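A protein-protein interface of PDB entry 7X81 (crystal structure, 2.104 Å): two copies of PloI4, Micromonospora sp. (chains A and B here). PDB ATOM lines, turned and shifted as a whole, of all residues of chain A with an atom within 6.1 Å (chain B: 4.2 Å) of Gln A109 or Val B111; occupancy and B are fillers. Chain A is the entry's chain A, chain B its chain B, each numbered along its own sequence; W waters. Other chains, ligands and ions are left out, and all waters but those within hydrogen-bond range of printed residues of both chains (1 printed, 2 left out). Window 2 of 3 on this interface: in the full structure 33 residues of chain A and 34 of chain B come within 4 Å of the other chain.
Water W1 lies within hydrogen-bond range of the backbone carbonyl oxygen of Val B111 (2.8 Å), the backbone carbonyl oxygen of Gly A117 (2.9 Å) and the side-chain hydroxyl of Ser A119 (3.1 Å).
Of chain B, only Thr B90, Gln B109 and Val B111 come within 4 Å of Gln A109. Val B111 touches one residue of chain A. Of the printed residues of chain A, Gln B109 touches Thr A90 (3.4 Å), Gln A109 (3.7 Å) and Val A111 (3.6 Å). Of the printed residues of chain B, Thr A90 touches Gln B109. Leu A118 touches none of the printed residues of chain B. The nearest residue of chain A that does not touch Val B111 is Ser A119 (4.6 Å).
Hydrophobic or aromatic side chains of chain B within 4 Å of the printed part of chain A: Val B111. Along chain B the printed residues that touch a printed residue of chain A span positions 90 to 116. Of the 16 printed residues of chain A, 4 touch a printed residue of chain B. Hydrophobic or aromatic side chains of chain A within 4 Å of the printed part of chain B: Val A111. Among the printed residues, no Asp or Glu carboxylate lies within 4 Å of a Lys or Arg side-chain nitrogen of the other chain.
Among the printed residues, merely in contact across the chains: Gln A109 with Thr B90 (3.4 Å), Thr A90 with Gln B109 (3.4 Å), Gln A109 with Val B111 (3.5 Å), Gly A117 with Arg B116 (3.5 Å), Val A111 with Gln B109 (3.6 Å) and Gln A109 with Gln B109 (3.7 Å).
O of Arg A88 sits at hydrogen-bond distance from N of Val A111 (2.9 Å). The side-chain hydroxyl (OG1) of Thr A90 lies within hydrogen-bond range of the side-chain amide oxygen (OE1) of Gln A109, 2.6 Å away. N of Gly A117 lies within hydrogen-bond range of O of Gly A110, 3.2 Å away. The backbone carbonyl oxygen (O) of Arg B88 sits at hydrogen-bond distance from the backbone NH (N) of Val B111 (3.1 Å). N of Gln B109 sits at hydrogen-bond distance from O of Thr B90 (2.8 Å). NE of Arg B116 lies within hydrogen-bond range of O of Val B111, 3.2 Å away.
Thr A90 touches Gln B109, and with the chains exchanged Gln A109 touches Thr B90. Gln A109 touches its own counterpart, Gln B109. Gln A109 touches Val B111, and with the chains exchanged Val A111 touches Gln B109. Of the 6 pairs that touch across the chains among the printed residues, 5 have their exchanged pair printed and touching as well.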
ATOM      1  N   ARG A  88      -7.126   8.032  -9.594  1.00  0.00           N
ATOM      2  CA  ARG A  88      -5.803   7.528  -9.886  1.00  0.00           C
ATOM      3  C   ARG A  88      -5.467   7.709 -11.356  1.00  0.00           C
ATOM      4  O   ARG A  88      -6.320   7.513 -12.229  1.00  0.00           O
ATOM      5  CB  ARG A  88      -5.704   6.051  -9.480  1.00  0.00           C
ATOM      6  CG  ARG A  88      -4.379   5.432  -9.911  1.00  0.00           C
ATOM      7  CD  ARG A  88      -4.231   4.056  -9.259  1.00  0.00           C
ATOM      8  NE  ARG A  88      -3.977   4.152  -7.833  1.00  0.00           N
ATOM      9  CZ  ARG A  88      -3.662   3.121  -7.060  1.00  0.00           C
ATOM     10  NH1 ARG A  88      -3.590   1.911  -7.587  1.00  0.00           N
ATOM     11  NH2 ARG A  88      -3.427   3.306  -5.765  1.00  0.00           N
ATOM     12  N   VAL A  89      -4.205   8.037 -11.611  1.00  0.00           N
ATOM     13  CA  VAL A  89      -3.630   8.145 -12.943  1.00  0.00           C
ATOM     14  C   VAL A  89      -2.395   7.258 -12.983  1.00  0.00           C
ATOM     15  O   VAL A  89      -1.483   7.449 -12.178  1.00  0.00           O
ATOM     16  CB  VAL A  89      -3.242   9.591 -13.277  1.00  0.00           C
ATOM     17  CG1 VAL A  89      -2.555   9.674 -14.616  1.00  0.00           C
ATOM     18  CG2 VAL A  89      -4.519  10.475 -13.190  1.00  0.00           C
ATOM     19  N   THR A  90      -2.389   6.262 -13.872  1.00  0.00           N
ATOM     20  CA  THR A  90      -1.175   5.481 -14.040  1.00  0.00           C
ATOM     21  C   THR A  90      -0.285   6.129 -15.092  1.00  0.00           C
ATOM     22  O   THR A  90      -0.761   6.843 -15.978  1.00  0.00           O
ATOM     23  CB  THR A  90      -1.502   4.044 -14.464  1.00  0.00           C
ATOM     24  OG1 THR A  90      -2.355   4.045 -15.619  1.00  0.00           O
ATOM     25  CG2 THR A  90      -2.219   3.327 -13.358  1.00  0.00           C
ATOM     26  N   TRP A  91       1.032   5.841 -15.013  1.00  0.00           N
ATOM     27  CA  TRP A  91       1.953   6.328 -16.037  1.00  0.00           C
ATOM     28  C   TRP A  91       3.165   5.408 -16.112  1.00  0.00           C
ATOM     29  O   TRP A  91       3.680   4.922 -15.085  1.00  0.00           O
ATOM     30  CB  TRP A  91       2.377   7.791 -15.790  1.00  0.00           C
ATOM     31  CG  TRP A  91       2.789   8.220 -14.369  1.00  0.00           C
ATOM     32  CD1 TRP A  91       1.977   8.560 -13.373  1.00  0.00           C
ATOM     33  CD2 TRP A  91       4.122   8.447 -13.881  1.00  0.00           C
ATOM     34  NE1 TRP A  91       2.679   8.977 -12.273  1.00  0.00           N
ATOM     35  CE2 TRP A  91       4.006   8.886 -12.546  1.00  0.00           C
ATOM     36  CE3 TRP A  91       5.397   8.261 -14.413  1.00  0.00           C
ATOM     37  CZ2 TRP A  91       5.124   9.148 -11.729  1.00  0.00           C
ATOM     38  CZ3 TRP A  91       6.497   8.552 -13.614  1.00  0.00           C
ATOM     39  CH2 TRP A  91       6.352   8.987 -12.290  1.00  0.00           C
ATOM     40  N   SER A  92       3.576   5.124 -17.346  1.00  0.00           N
ATOM     41  CA  SER A  92       4.633   4.153 -17.578  1.00  0.00           C
ATOM     42  C   SER A  92       5.234   4.360 -18.958  1.00  0.00           C
ATOM     43  O   SER A  92       4.526   4.691 -19.908  1.00  0.00           O
ATOM     44  CB  SER A  92       4.080   2.725 -17.452  1.00  0.00           C
ATOM     45  OG  SER A  92       5.079   1.760 -17.722  1.00  0.00           O
ATOM     46  N   PRO A 107       3.715   8.158 -21.297  1.00  0.00           N
ATOM     47  CA  PRO A 107       2.246   8.209 -21.386  1.00  0.00           C
ATOM     48  C   PRO A 107       1.594   7.971 -20.043  1.00  0.00           C
ATOM     49  O   PRO A 107       2.123   7.258 -19.197  1.00  0.00           O
ATOM     50  CB  PRO A 107       1.882   7.086 -22.369  1.00  0.00           C
ATOM     51  CG  PRO A 107       3.188   6.887 -23.213  1.00  0.00           C
ATOM     52  CD  PRO A 107       4.310   7.166 -22.226  1.00  0.00           C
ATOM     53  N   ALA A 108       0.411   8.555 -19.878  1.00  0.00           N
ATOM     54  CA  ALA A 108      -0.371   8.461 -18.664  1.00  0.00           C
ATOM     55  C   ALA A 108      -1.800   8.073 -18.999  1.00  0.00           C
ATOM     56  O   ALA A 108      -2.342   8.494 -20.030  1.00  0.00           O
ATOM     57  CB  ALA A 108      -0.397   9.826 -17.909  1.00  0.00           C
ATOM     58  N   GLN A 109      -2.406   7.314 -18.100  1.00  0.00           N
ATOM     59  CA  GLN A 109      -3.807   6.926 -18.231  1.00  0.00           C
ATOM     60  C   GLN A 109      -4.614   7.181 -16.962  1.00  0.00           C
ATOM     61  O   GLN A 109      -4.276   6.684 -15.881  1.00  0.00           O
ATOM     62  CB  GLN A 109      -3.937   5.435 -18.591  1.00  0.00           C
ATOM     63  CG  GLN A 109      -2.964   4.995 -19.709  1.00  0.00           C
ATOM     64  CD  GLN A 109      -1.551   4.775 -19.207  1.00  0.00           C
ATOM     65  OE1 GLN A 109      -1.339   4.398 -18.036  1.00  0.00           O
ATOM     66  NE2 GLN A 109      -0.564   5.023 -20.076  1.00  0.00           N
ATOM     67  N   GLY A 110      -5.733   7.891 -17.107  1.00  0.00           N
ATOM     68  CA  GLY A 110      -6.656   8.054 -15.987  1.00  0.00           C
ATOM     69  C   GLY A 110      -7.488   6.798 -15.814  1.00  0.00           C
ATOM     70  O   GLY A 110      -8.036   6.262 -16.783  1.00  0.00           O
ATOM     71  N   VAL A 111      -7.521   6.267 -14.601  1.00  0.00           N
ATOM     72  CA  VAL A 111      -8.221   5.012 -14.391  1.00  0.00           C
ATOM     73  C   VAL A 111      -9.423   5.147 -13.462  1.00  0.00           C
ATOM     74  O   VAL A 111     -10.300   4.274 -13.507  1.00  0.00           O
ATOM     75  CB  VAL A 111      -7.274   3.911 -13.883  1.00  0.00           C
ATOM     76  CG1 VAL A 111      -6.140   3.720 -14.854  1.00  0.00           C
ATOM     77  CG2 VAL A 111      -6.730   4.280 -12.557  1.00  0.00           C
ATOM     78  N   TYR A 115     -10.471  11.355 -13.687  1.00  0.00           N
ATOM     79  CA  TYR A 115      -9.474  11.054 -14.700  1.00  0.00           C
ATOM     80  C   TYR A 115      -9.869   9.902 -15.595  1.00  0.00           C
ATOM     81  O   TYR A 115      -9.231   9.732 -16.634  1.00  0.00           O
ATOM     82  CB  TYR A 115      -8.113  10.731 -14.029  1.00  0.00           C
ATOM     83  CG  TYR A 115      -7.821  11.742 -12.980  1.00  0.00           C
ATOM     84  CD1 TYR A 115      -7.356  12.967 -13.336  1.00  0.00           C
ATOM     85  CD2 TYR A 115      -8.092  11.491 -11.658  1.00  0.00           C
ATOM     86  CE1 TYR A 115      -7.130  13.944 -12.397  1.00  0.00           C
ATOM     87  CE2 TYR A 115      -7.913  12.457 -10.692  1.00  0.00           C
ATOM     88  CZ  TYR A 115      -7.422  13.695 -11.069  1.00  0.00           C
ATOM     89  OH  TYR A 115      -7.232  14.673 -10.155  1.00  0.00           O
ATOM     90  N   GLY A 117     -10.769   7.144 -18.132  1.00  0.00           N
ATOM     91  CA  GLY A 117     -10.987   7.170 -19.566  1.00  0.00           C
ATOM     92  C   GLY A 117     -10.253   8.273 -20.305  1.00  0.00           C
ATOM     93  O   GLY A 117     -10.426   8.415 -21.513  1.00  0.00           O
ATOM     94  N   LEU A 118      -9.451   9.066 -19.623  1.00  0.00           N
ATOM     95  CA  LEU A 118      -8.700  10.128 -20.267  1.00  0.00           C
ATOM     96  C   LEU A 118      -7.255   9.660 -20.342  1.00  0.00           C
ATOM     97  O   LEU A 118      -6.788   8.944 -19.458  1.00  0.00           O
ATOM     98  CB  LEU A 118      -8.774  11.444 -19.511  1.00  0.00           C
ATOM     99  CG  LEU A 118     -10.154  11.938 -19.095  1.00  0.00           C
ATOM    100  CD1 LEU A 118     -10.039  13.189 -18.254  1.00  0.00           C
ATOM    101  CD2 LEU A 118     -10.988  12.226 -20.312  1.00  0.00           C
ATOM    102  N   SER A 119      -6.549  10.100 -21.374  1.00  0.00           N
ATOM    103  CA  SER A 119      -5.168   9.693 -21.591  1.00  0.00           C
ATOM    104  C   SER A 119      -4.355  10.909 -22.006  1.00  0.00           C
ATOM    105  O   SER A 119      -4.897  11.885 -22.523  1.00  0.00           O
ATOM    106  CB  SER A 119      -5.091   8.607 -22.676  1.00  0.00           C
ATOM    107  OG  SER A 119      -5.739   9.114 -23.826  1.00  0.00           O
ATOM    108  N   GLY A 120      -3.039  10.823 -21.793  1.00  0.00           N
ATOM    109  CA  GLY A 120      -2.105  11.846 -22.193  1.00  0.00           C
ATOM    110  C   GLY A 120      -0.694  11.586 -21.697  1.00  0.00           C
ATOM    111  O   GLY A 120      -0.128  10.510 -21.951  1.00  0.00           O
ATOM    112  N   LEU A 143      -4.136  15.375 -19.575  1.00  0.00           N
ATOM    113  CA  LEU A 143      -5.020  14.297 -19.978  1.00  0.00           C
ATOM    114  C   LEU A 143      -6.130  14.864 -20.831  1.00  0.00           C
ATOM    115  O   LEU A 143      -6.662  15.925 -20.522  1.00  0.00           O
ATOM    116  CB  LEU A 143      -5.677  13.578 -18.768  1.00  0.00           C
ATOM    117  CG  LEU A 143      -4.783  12.837 -17.794  1.00  0.00           C
ATOM    118  CD1 LEU A 143      -5.612  12.272 -16.697  1.00  0.00           C
ATOM    119  CD2 LEU A 143      -4.013  11.728 -18.567  1.00  0.00           C
ATOM    120  N   ARG B  88      -6.869   0.163 -27.663  1.00  0.00           N
ATOM    121  CA  ARG B  88      -5.553  -0.045 -27.074  1.00  0.00           C
ATOM    122  C   ARG B  88      -5.732  -0.290 -25.584  1.00  0.00           C
ATOM    123  O   ARG B  88      -6.644   0.248 -24.967  1.00  0.00           O
ATOM    124  CB  ARG B  88      -4.673   1.180 -27.318  1.00  0.00           C
ATOM    125  CG  ARG B  88      -3.346   1.153 -26.625  1.00  0.00           C
ATOM    126  CD  ARG B  88      -2.490   2.331 -27.088  1.00  0.00           C
ATOM    127  NE  ARG B  88      -1.935   2.089 -28.407  1.00  0.00           N
ATOM    128  CZ  ARG B  88      -1.324   3.002 -29.147  1.00  0.00           C
ATOM    129  NH1 ARG B  88      -1.188   4.232 -28.683  1.00  0.00           N
ATOM    130  NH2 ARG B  88      -0.858   2.686 -30.355  1.00  0.00           N
ATOM    131  N   THR B  90      -3.084  -0.422 -22.240  1.00  0.00           N
ATOM    132  CA  THR B  90      -1.716  -0.334 -21.750  1.00  0.00           C
ATOM    133  C   THR B  90      -1.549  -1.297 -20.575  1.00  0.00           C
ATOM    134  O   THR B  90      -2.520  -1.623 -19.870  1.00  0.00           O
ATOM    135  CB  THR B  90      -1.340   1.098 -21.339  1.00  0.00           C
ATOM    136  OG1 THR B  90      -2.327   1.724 -20.484  1.00  0.00           O
ATOM    137  CG2 THR B  90      -1.216   1.907 -22.544  1.00  0.00           C
ATOM    138  N   GLN B 109      -4.735  -1.056 -18.302  1.00  0.00           N
ATOM    139  CA  GLN B 109      -5.629   0.088 -18.392  1.00  0.00           C
ATOM    140  C   GLN B 109      -6.133   0.181 -19.819  1.00  0.00           C
ATOM    141  O   GLN B 109      -5.347   0.372 -20.738  1.00  0.00           O
ATOM    142  CB  GLN B 109      -4.925   1.406 -17.995  1.00  0.00           C
ATOM    143  CG  GLN B 109      -4.169   1.337 -16.690  1.00  0.00           C
ATOM    144  CD  GLN B 109      -2.778   0.682 -16.805  1.00  0.00           C
ATOM    145  OE1 GLN B 109      -2.084   0.805 -17.816  1.00  0.00           O
ATOM    146  NE2 GLN B 109      -2.381  -0.021 -15.749  1.00  0.00           N
ATOM    147  N   GLY B 110      -7.438   0.054 -20.015  1.00  0.00           N
ATOM    148  CA  GLY B 110      -7.996   0.333 -21.327  1.00  0.00           C
ATOM    149  C   GLY B 110      -8.040   1.829 -21.611  1.00  0.00           C
ATOM    150  O   GLY B 110      -8.537   2.613 -20.790  1.00  0.00           O
ATOM    151  N   VAL B 111      -7.576   2.223 -22.803  1.00  0.00           N
ATOM    152  CA  VAL B 111      -7.465   3.641 -23.138  1.00  0.00           C
ATOM    153  C   VAL B 111      -8.214   4.070 -24.399  1.00  0.00           C
ATOM    154  O   VAL B 111      -8.337   5.289 -24.642  1.00  0.00           O
ATOM    155  CB  VAL B 111      -5.990   4.090 -23.238  1.00  0.00           C
ATOM    156  CG1 VAL B 111      -5.188   3.607 -22.010  1.00  0.00           C
ATOM    157  CG2 VAL B 111      -5.329   3.584 -24.462  1.00  0.00           C
ATOM    158  N   SER B 112      -8.728   3.167 -25.212  1.00  0.00           N
ATOM    159  CA  SER B 112      -9.459   3.602 -26.401  1.00  0.00           C
ATOM    160  C   SER B 112     -10.375   2.482 -26.858  1.00  0.00           C
ATOM    161  O   SER B 112     -10.266   1.339 -26.406  1.00  0.00           O
ATOM    162  CB  SER B 112      -8.512   4.006 -27.544  1.00  0.00           C
ATOM    163  OG  SER B 112      -7.758   2.907 -28.060  1.00  0.00           O
ATOM    164  N   ARG B 116     -11.870   1.718 -23.388  1.00  0.00           N
ATOM    165  CA  ARG B 116     -11.595   3.010 -22.762  1.00  0.00           C
ATOM    166  C   ARG B 116     -12.290   3.083 -21.410  1.00  0.00           C
ATOM    167  O   ARG B 116     -13.489   2.836 -21.300  1.00  0.00           O
ATOM    168  CB  ARG B 116     -12.052   4.164 -23.681  1.00  0.00           C
ATOM    169  CG  ARG B 116     -11.851   5.621 -23.168  1.00  0.00           C
ATOM    170  CD  ARG B 116     -12.132   6.745 -24.242  1.00  0.00           C
ATOM    171  NE  ARG B 116     -10.968   7.023 -25.115  1.00  0.00           N
ATOM    172  CZ  ARG B 116     -10.824   8.104 -25.904  1.00  0.00           C
ATOM    173  NH1 ARG B 116      -9.754   8.232 -26.677  1.00  0.00           N
ATOM    174  NH2 ARG B 116     -11.745   9.067 -25.932  1.00  0.00           N
HETATM  175  O   HOH W   1      -8.064   7.374 -22.752  1.00  0.00           O
